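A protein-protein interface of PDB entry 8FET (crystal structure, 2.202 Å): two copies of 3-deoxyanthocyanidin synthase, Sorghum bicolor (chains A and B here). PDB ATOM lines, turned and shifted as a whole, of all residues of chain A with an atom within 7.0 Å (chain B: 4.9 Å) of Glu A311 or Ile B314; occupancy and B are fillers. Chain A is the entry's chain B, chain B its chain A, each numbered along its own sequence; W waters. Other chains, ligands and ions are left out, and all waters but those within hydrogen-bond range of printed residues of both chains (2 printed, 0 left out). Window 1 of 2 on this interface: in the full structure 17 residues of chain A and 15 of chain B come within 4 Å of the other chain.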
ATOM      1  N   VAL A 151      20.530  -0.308  17.474  1.00  0.00           N
ATOM      2  CA  VAL A 151      19.142  -0.103  17.845  1.00  0.00           C
ATOM      3  C   VAL A 151      18.732  -1.374  18.556  1.00  0.00           C
ATOM      4  O   VAL A 151      18.711  -2.449  17.945  1.00  0.00           O
ATOM      5  CB  VAL A 151      18.245   0.169  16.625  1.00  0.00           C
ATOM      6  CG1 VAL A 151      16.878   0.639  17.060  1.00  0.00           C
ATOM      7  CG2 VAL A 151      18.864   1.206  15.732  1.00  0.00           C
ATOM      8  N   GLU A 154      12.931  -5.378  21.567  1.00  0.00           N
ATOM      9  CA  GLU A 154      12.390  -6.167  22.663  1.00  0.00           C
ATOM     10  C   GLU A 154      12.964  -7.581  22.743  1.00  0.00           C
ATOM     11  O   GLU A 154      12.661  -8.289  23.704  1.00  0.00           O
ATOM     12  CB  GLU A 154      10.870  -6.235  22.538  1.00  0.00           C
ATOM     13  CG  GLU A 154      10.149  -4.939  22.888  1.00  0.00           C
ATOM     14  CD  GLU A 154      10.163  -3.914  21.755  1.00  0.00           C
ATOM     15  OE1 GLU A 154      10.761  -4.176  20.684  1.00  0.00           O
ATOM     16  OE2 GLU A 154       9.578  -2.825  21.948  1.00  0.00           O
ATOM     17  N   ILE A 269       8.963  -1.757  24.656  1.00  0.00           N
ATOM     18  CA  ILE A 269       9.725  -0.573  25.034  1.00  0.00           C
ATOM     19  C   ILE A 269       8.796   0.632  25.039  1.00  0.00           C
ATOM     20  O   ILE A 269       7.896   0.750  24.191  1.00  0.00           O
ATOM     21  CB  ILE A 269      10.915  -0.381  24.075  1.00  0.00           C
ATOM     22  CG1 ILE A 269      11.961  -1.481  24.292  1.00  0.00           C
ATOM     23  CG2 ILE A 269      11.553   0.994  24.262  1.00  0.00           C
ATOM     24  CD1 ILE A 269      12.977  -1.627  23.136  1.00  0.00           C
ATOM     25  N   MET A 308      17.112   2.938  21.468  1.00  0.00           N
ATOM     26  CA  MET A 308      15.963   2.071  21.661  1.00  0.00           C
ATOM     27  C   MET A 308      15.059   2.108  20.439  1.00  0.00           C
ATOM     28  O   MET A 308      14.841   3.169  19.845  1.00  0.00           O
ATOM     29  CB  MET A 308      15.164   2.478  22.903  1.00  0.00           C
ATOM     30  CG  MET A 308      15.886   2.243  24.217  1.00  0.00           C
ATOM     31  SD  MET A 308      16.137   0.496  24.590  1.00  0.00           S
ATOM     32  CE  MET A 308      17.901   0.468  24.780  1.00  0.00           C
ATOM     33  N   SER A 309      14.531   0.947  20.071  1.00  0.00           N
ATOM     34  CA  SER A 309      13.526   0.882  19.027  1.00  0.00           C
ATOM     35  C   SER A 309      12.182   1.340  19.567  1.00  0.00           C
ATOM     36  O   SER A 309      11.769   0.939  20.657  1.00  0.00           O
ATOM     37  CB  SER A 309      13.389  -0.537  18.496  1.00  0.00           C
ATOM     38  OG  SER A 309      12.166  -0.647  17.790  1.00  0.00           O
ATOM     39  N   LEU A 310      11.482   2.159  18.783  1.00  0.00           N
ATOM     40  CA  LEU A 310      10.174   2.673  19.168  1.00  0.00           C
ATOM     41  C   LEU A 310       9.035   1.984  18.430  1.00  0.00           C
ATOM     42  O   LEU A 310       7.878   2.381  18.585  1.00  0.00           O
ATOM     43  CB  LEU A 310      10.105   4.183  18.916  1.00  0.00           C
ATOM     44  CG  LEU A 310      11.291   4.982  19.463  1.00  0.00           C
ATOM     45  CD1 LEU A 310      11.078   6.468  19.287  1.00  0.00           C
ATOM     46  CD2 LEU A 310      11.512   4.661  20.920  1.00  0.00           C
ATOM     47  N   GLU A 311       9.322   0.961  17.638  1.00  0.00           N
ATOM     48  CA  GLU A 311       8.348   0.544  16.645  1.00  0.00           C
ATOM     49  C   GLU A 311       7.238  -0.339  17.187  1.00  0.00           C
ATOM     50  O   GLU A 311       6.162  -0.370  16.584  1.00  0.00           O
ATOM     51  CB  GLU A 311       9.061  -0.165  15.507  1.00  0.00           C
ATOM     52  CG  GLU A 311       9.958   0.795  14.772  1.00  0.00           C
ATOM     53  CD  GLU A 311      10.675   0.148  13.635  1.00  0.00           C
ATOM     54  OE1 GLU A 311      10.237  -0.950  13.232  1.00  0.00           O
ATOM     55  OE2 GLU A 311      11.680   0.722  13.155  1.00  0.00           O
ATOM     56  N   LYS A 312       7.441  -1.059  18.291  1.00  0.00           N
ATOM     57  CA  LYS A 312       6.443  -2.073  18.627  1.00  0.00           C
ATOM     58  C   LYS A 312       5.110  -1.441  19.018  1.00  0.00           C
ATOM     59  O   LYS A 312       4.052  -1.838  18.509  1.00  0.00           O
ATOM     60  CB  LYS A 312       6.945  -3.004  19.726  1.00  0.00           C
ATOM     61  CG  LYS A 312       6.069  -4.250  19.856  1.00  0.00           C
ATOM     62  CD  LYS A 312       6.704  -5.301  20.765  1.00  0.00           C
ATOM     63  CE  LYS A 312       5.707  -6.406  21.103  1.00  0.00           C
ATOM     64  NZ  LYS A 312       6.327  -7.490  21.935  1.00  0.00           N
ATOM     65  N   LEU A 313       5.130  -0.453  19.917  1.00  0.00           N
ATOM     66  CA  LEU A 313       3.870   0.187  20.299  1.00  0.00           C
ATOM     67  C   LEU A 313       3.243   0.906  19.109  1.00  0.00           C
ATOM     68  O   LEU A 313       2.017   0.899  18.947  1.00  0.00           O
ATOM     69  CB  LEU A 313       4.087   1.165  21.455  1.00  0.00           C
ATOM     70  CG  LEU A 313       4.135   0.619  22.883  1.00  0.00           C
ATOM     71  CD1 LEU A 313       4.640   1.702  23.856  1.00  0.00           C
ATOM     72  CD2 LEU A 313       2.768   0.086  23.304  1.00  0.00           C
ATOM     73  N   ILE A 314       4.068   1.539  18.269  1.00  0.00           N
ATOM     74  CA  ILE A 314       3.544   2.245  17.099  1.00  0.00           C
ATOM     75  C   ILE A 314       2.889   1.255  16.144  1.00  0.00           C
ATOM     76  O   ILE A 314       1.737   1.430  15.731  1.00  0.00           O
ATOM     77  CB  ILE A 314       4.663   3.057  16.413  1.00  0.00           C
ATOM     78  CG1 ILE A 314       5.325   4.036  17.402  1.00  0.00           C
ATOM     79  CG2 ILE A 314       4.141   3.803  15.190  1.00  0.00           C
ATOM     80  CD1 ILE A 314       4.347   4.842  18.189  1.00  0.00           C
ATOM     81  N   ARG A 315       3.601   0.170  15.824  1.00  0.00           N
ATOM     82  CA  ARG A 315       3.067  -0.873  14.951  1.00  0.00           C
ATOM     83  C   ARG A 315       1.678  -1.326  15.383  1.00  0.00           C
ATOM     84  O   ARG A 315       0.804  -1.577  14.546  1.00  0.00           O
ATOM     85  CB  ARG A 315       4.017  -2.067  14.946  1.00  0.00           C
ATOM     86  CG  ARG A 315       4.829  -2.141  13.724  1.00  0.00           C
ATOM     87  CD  ARG A 315       5.804  -3.277  13.802  1.00  0.00           C
ATOM     88  NE  ARG A 315       7.105  -2.884  13.276  1.00  0.00           N
ATOM     89  CZ  ARG A 315       7.323  -2.351  12.077  1.00  0.00           C
ATOM     90  NH1 ARG A 315       6.329  -2.127  11.213  1.00  0.00           N
ATOM     91  NH2 ARG A 315       8.570  -2.032  11.732  1.00  0.00           N
ATOM     92  N   GLU A 316       1.461  -1.466  16.678  1.00  0.00           N
ATOM     93  CA  GLU A 316       0.195  -1.980  17.165  1.00  0.00           C
ATOM     94  C   GLU A 316      -0.839  -0.893  17.402  1.00  0.00           C
ATOM     95  O   GLU A 316      -1.881  -1.177  17.991  1.00  0.00           O
ATOM     96  CB  GLU A 316       0.429  -2.789  18.439  1.00  0.00           C
ATOM     97  CG  GLU A 316       1.536  -3.792  18.239  1.00  0.00           C
ATOM     98  CD  GLU A 316       1.538  -4.885  19.276  1.00  0.00           C
ATOM     99  OE1 GLU A 316       0.595  -4.942  20.091  1.00  0.00           O
ATOM    100  OE2 GLU A 316       2.493  -5.687  19.262  1.00  0.00           O
ATOM    101  N   GLY A 317      -0.573   0.340  16.958  1.00  0.00           N
ATOM    102  CA  GLY A 317      -1.579   1.380  16.929  1.00  0.00           C
ATOM    103  C   GLY A 317      -1.478   2.446  17.999  1.00  0.00           C
ATOM    104  O   GLY A 317      -2.282   3.384  17.978  1.00  0.00           O
ATOM    105  N   ARG B 272      14.831   7.229   7.761  1.00  0.00           N
ATOM    106  CA  ARG B 272      15.209   6.293   8.822  1.00  0.00           C
ATOM    107  C   ARG B 272      16.175   6.823   9.879  1.00  0.00           C
ATOM    108  O   ARG B 272      15.944   6.619  11.074  1.00  0.00           O
ATOM    109  CB  ARG B 272      15.811   5.016   8.236  1.00  0.00           C
ATOM    110  CG  ARG B 272      15.930   3.892   9.269  1.00  0.00           C
ATOM    111  CD  ARG B 272      14.696   3.753  10.175  1.00  0.00           C
ATOM    112  NE  ARG B 272      14.937   2.829  11.287  1.00  0.00           N
ATOM    113  CZ  ARG B 272      15.404   3.181  12.482  1.00  0.00           C
ATOM    114  NH1 ARG B 272      15.700   4.442  12.770  1.00  0.00           N
ATOM    115  NH2 ARG B 272      15.560   2.248  13.418  1.00  0.00           N
ATOM    116  N   LEU B 310       8.262   9.230  11.366  1.00  0.00           N
ATOM    117  CA  LEU B 310       8.488   7.950  10.701  1.00  0.00           C
ATOM    118  C   LEU B 310       7.326   6.982  10.885  1.00  0.00           C
ATOM    119  O   LEU B 310       7.450   5.803  10.533  1.00  0.00           O
ATOM    120  CB  LEU B 310       9.782   7.307  11.215  1.00  0.00           C
ATOM    121  CG  LEU B 310      10.979   8.260  11.195  1.00  0.00           C
ATOM    122  CD1 LEU B 310      12.254   7.547  11.599  1.00  0.00           C
ATOM    123  CD2 LEU B 310      11.115   8.853   9.821  1.00  0.00           C
ATOM    124  N   GLU B 311       6.191   7.450  11.401  1.00  0.00           N
ATOM    125  CA  GLU B 311       5.217   6.523  11.948  1.00  0.00           C
ATOM    126  C   GLU B 311       4.264   5.922  10.919  1.00  0.00           C
ATOM    127  O   GLU B 311       3.732   4.837  11.167  1.00  0.00           O
ATOM    128  CB  GLU B 311       4.431   7.223  13.050  1.00  0.00           C
ATOM    129  CG  GLU B 311       5.337   7.765  14.149  1.00  0.00           C
ATOM    130  CD  GLU B 311       4.575   8.157  15.395  1.00  0.00           C
ATOM    131  OE1 GLU B 311       3.346   7.948  15.410  1.00  0.00           O
ATOM    132  OE2 GLU B 311       5.200   8.669  16.353  1.00  0.00           O
ATOM    133  N   LYS B 312       4.038   6.571   9.772  1.00  0.00           N
ATOM    134  CA  LYS B 312       2.958   6.113   8.894  1.00  0.00           C
ATOM    135  C   LYS B 312       3.276   4.763   8.258  1.00  0.00           C
ATOM    136  O   LYS B 312       2.457   3.841   8.300  1.00  0.00           O
ATOM    137  CB  LYS B 312       2.655   7.138   7.806  1.00  0.00           C
ATOM    138  CG  LYS B 312       1.223   7.012   7.313  1.00  0.00           C
ATOM    139  CD  LYS B 312       0.906   7.970   6.184  1.00  0.00           C
ATOM    140  CE  LYS B 312      -0.447   7.627   5.593  1.00  0.00           C
ATOM    141  NZ  LYS B 312      -0.860   8.619   4.573  1.00  0.00           N
ATOM    142  N   LEU B 313       4.437   4.646   7.615  1.00  0.00           N
ATOM    143  CA  LEU B 313       4.837   3.355   7.078  1.00  0.00           C
ATOM    144  C   LEU B 313       4.902   2.301   8.179  1.00  0.00           C
ATOM    145  O   LEU B 313       4.477   1.161   7.973  1.00  0.00           O
ATOM    146  CB  LEU B 313       6.187   3.469   6.370  1.00  0.00           C
ATOM    147  CG  LEU B 313       6.181   4.015   4.953  1.00  0.00           C
ATOM    148  CD1 LEU B 313       7.615   4.110   4.432  1.00  0.00           C
ATOM    149  CD2 LEU B 313       5.297   3.152   4.042  1.00  0.00           C
ATOM    150  N   ILE B 314       5.436   2.661   9.354  1.00  0.00           N
ATOM    151  CA  ILE B 314       5.604   1.683  10.439  1.00  0.00           C
ATOM    152  C   ILE B 314       4.249   1.206  10.939  1.00  0.00           C
ATOM    153  O   ILE B 314       4.023   0.007  11.153  1.00  0.00           O
ATOM    154  CB  ILE B 314       6.427   2.271  11.605  1.00  0.00           C
ATOM    155  CG1 ILE B 314       7.840   2.697  11.180  1.00  0.00           C
ATOM    156  CG2 ILE B 314       6.463   1.286  12.793  1.00  0.00           C
ATOM    157  CD1 ILE B 314       8.667   1.597  10.617  1.00  0.00           C
ATOM    158  N   ARG B 315       3.334   2.148  11.165  1.00  0.00           N
ATOM    159  CA  ARG B 315       2.016   1.801  11.664  1.00  0.00           C
ATOM    160  C   ARG B 315       1.296   0.868  10.698  1.00  0.00           C
ATOM    161  O   ARG B 315       0.461   0.053  11.112  1.00  0.00           O
ATOM    162  CB  ARG B 315       1.220   3.088  11.903  1.00  0.00           C
ATOM    163  CG  ARG B 315      -0.107   2.889  12.558  1.00  0.00           C
ATOM    164  CD  ARG B 315      -0.719   4.203  13.036  1.00  0.00           C
ATOM    165  NE  ARG B 315       0.247   5.187  13.519  1.00  0.00           N
ATOM    166  CZ  ARG B 315       0.692   5.264  14.772  1.00  0.00           C
ATOM    167  NH1 ARG B 315       0.420   4.316  15.669  1.00  0.00           N
ATOM    168  NH2 ARG B 315       1.424   6.317  15.137  1.00  0.00           N
ATOM    169  N   GLU B 316       1.609   0.961   9.416  1.00  0.00           N
ATOM    170  CA  GLU B 316       0.944   0.134   8.428  1.00  0.00           C
ATOM    171  C   GLU B 316       1.682  -1.168   8.149  1.00  0.00           C
ATOM    172  O   GLU B 316       1.267  -1.915   7.259  1.00  0.00           O
ATOM    173  CB  GLU B 316       0.734   0.927   7.138  1.00  0.00           C
ATOM    174  CG  GLU B 316      -0.642   1.571   7.101  1.00  0.00           C
ATOM    175  CD  GLU B 316      -0.746   2.717   6.117  1.00  0.00           C
ATOM    176  OE1 GLU B 316      -0.651   2.464   4.900  1.00  0.00           O
ATOM    177  OE2 GLU B 316      -0.929   3.867   6.566  1.00  0.00           O
ATOM    178  N   GLY B 317       2.759  -1.461   8.887  1.00  0.00           N
ATOM    179  CA  GLY B 317       3.392  -2.764   8.835  1.00  0.00           C
ATOM    180  C   GLY B 317       4.691  -2.844   8.070  1.00  0.00           C
ATOM    181  O   GLY B 317       5.266  -3.928   7.988  1.00  0.00           O
ATOM    182  N   PHE B 318       5.174  -1.745   7.506  1.00  0.00           N
ATOM    183  CA  PHE B 318       6.454  -1.774   6.816  1.00  0.00           C
ATOM    184  C   PHE B 318       7.601  -1.885   7.815  1.00  0.00           C
ATOM    185  O   PHE B 318       7.512  -1.389   8.940  1.00  0.00           O
ATOM    186  CB  PHE B 318       6.643  -0.507   5.987  1.00  0.00           C
ATOM    187  CG  PHE B 318       7.941  -0.466   5.243  1.00  0.00           C
ATOM    188  CD1 PHE B 318       8.117  -1.229   4.098  1.00  0.00           C
ATOM    189  CD2 PHE B 318       8.975   0.342   5.679  1.00  0.00           C
ATOM    190  CE1 PHE B 318       9.311  -1.187   3.398  1.00  0.00           C
ATOM    191  CE2 PHE B 318      10.170   0.395   4.988  1.00  0.00           C
ATOM    192  CZ  PHE B 318      10.342  -0.375   3.840  1.00  0.00           C
ATOM    193  N   TYR B 320      11.845  -1.200   8.025  1.00  0.00           N
ATOM    194  CA  TYR B 320      13.147  -0.824   7.489  1.00  0.00           C
ATOM    195  C   TYR B 320      14.195  -1.867   7.876  1.00  0.00           C
ATOM    196  O   TYR B 320      14.179  -2.405   8.986  1.00  0.00           O
ATOM    197  CB  TYR B 320      13.567   0.555   8.011  1.00  0.00           C
ATOM    198  CG  TYR B 320      12.721   1.736   7.524  1.00  0.00           C
ATOM    199  CD1 TYR B 320      11.494   2.032   8.105  1.00  0.00           C
ATOM    200  CD2 TYR B 320      13.162   2.558   6.488  1.00  0.00           C
ATOM    201  CE1 TYR B 320      10.713   3.128   7.660  1.00  0.00           C
ATOM    202  CE2 TYR B 320      12.399   3.647   6.042  1.00  0.00           C
ATOM    203  CZ  TYR B 320      11.173   3.927   6.634  1.00  0.00           C
ATOM    204  OH  TYR B 320      10.419   5.001   6.194  1.00  0.00           O
ATOM    205  N   ASN B 323      18.920   0.244   9.631  1.00  0.00           N
ATOM    206  CA  ASN B 323      18.407   1.009  10.752  1.00  0.00           C
ATOM    207  C   ASN B 323      19.456   1.798  11.505  1.00  0.00           C
ATOM    208  O   ASN B 323      19.096   2.608  12.358  1.00  0.00           O
ATOM    209  CB  ASN B 323      17.686   0.080  11.724  1.00  0.00           C
ATOM    210  CG  ASN B 323      16.517  -0.610  11.079  1.00  0.00           C
ATOM    211  OD1 ASN B 323      15.501   0.024  10.779  1.00  0.00           O
ATOM    212  ND2 ASN B 323      16.644  -1.914  10.858  1.00  0.00           N
HETATM  213  O   HOH W   1      -1.226   0.058  13.364  1.00  0.00           O
HETATM  214  O   HOH W   2      11.218  -0.686  10.395  1.00  0.00           O
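Hydrophobic or aromatic side chains of chain A within 4 Å of the printed part of chain B: Val A151 and Ile A314.
Among the printed residues, merely in contact across the chains: Val A151 with Asn B323, Glu A311 with Ile B314, Arg A315 with Arg B315, Arg A315 with Gly B317 and Gly A317 with Arg B315.
The backbone carbonyl oxygen (O) of Leu B313 sits at hydrogen-bond distance from the backbone NH (N) of Phe B318, at 3.0 Å.
The side-chain carboxylate of Glu B311 is in salt-bridge range of the guanidinium group of Arg B315 (2.5 Å).
The side-chain carboxylate (OE1) of Glu A311 is in salt-bridge range of the guanidinium group (NH2) of Arg A315, at 2.5 Å.
The guanidinium group (NE) of Arg B272 lies within hydrogen-bond range of the side-chain amide oxygen (OD1) of Asn B323 (2.9 Å).
The backbone carbonyl oxygen (O) of Tyr B320 lies within hydrogen-bond range of the side-chain amide nitrogen (ND2) of Asn B323 (3.1 Å).
The backbone NH of Glu A311 is in hydrogen-bond range of the side-chain hydroxyl of Ser A309 (3.3 Å).
Glu A311 touches Ile B314, but with the chains exchanged Ile A314 does not touch Glu B311 (4.04 Å).
Ile A314 touches Arg B315, and with the chains exchanged Arg A315 touches Ile B314.
Arg A315 touches its own counterpart, Arg B315.
Arg A315 touches Gly B317, and with the chains exchanged Gly A317 touches Arg B315.
8 positions are printed for both chains.
Of the 8 pairs that touch across the chains among the printed residues, 5 have their exchanged pair printed and touching as well.
Water W2 lies within hydrogen-bond range of the backbone NH of Tyr B320 (2.5 Å), the side-chain carboxylate of Glu A311 (3.0 Å) and the guanidinium group of Arg A315 (3.3 Å).
Water W1 lies within hydrogen-bond range of the backbone carbonyl oxygen (O) of Arg B315 (2.8 Å) and the backbone carbonyl oxygen (O) of Arg A315 (2.9 Å).
Glu A311 touches just one residue of chain B: Ile B314 (3.9 Å).
Printed residues of chain B within 4 Å of Arg A315: Ile B314, Arg B315, Gly B317 and Phe B318.
Printed residues of chain A within 4 Å of Phe B318: Arg A315 (2.7 Å).
Of the printed residues of chain A, Arg B315 touches Ile A314 (3.2 Å), Arg A315 (3.8 Å) and Gly A317 (3.5 Å).
Tyr B320 touches none of the printed residues of chain A.
The guanidinium group (NH1) of Arg B315 is in hydrogen-bond range of the backbone carbonyl oxygen (O) of Ile A314 (3.2 Å).
The backbone carbonyl oxygen of Phe B318 sits at hydrogen-bond distance from the guanidinium group of Arg A315, 2.7 Å away.
The guanidinium group (NH1) of Arg A315 is in hydrogen-bond range of the backbone carbonyl oxygen (O) of Ile B314 (3.1 Å).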
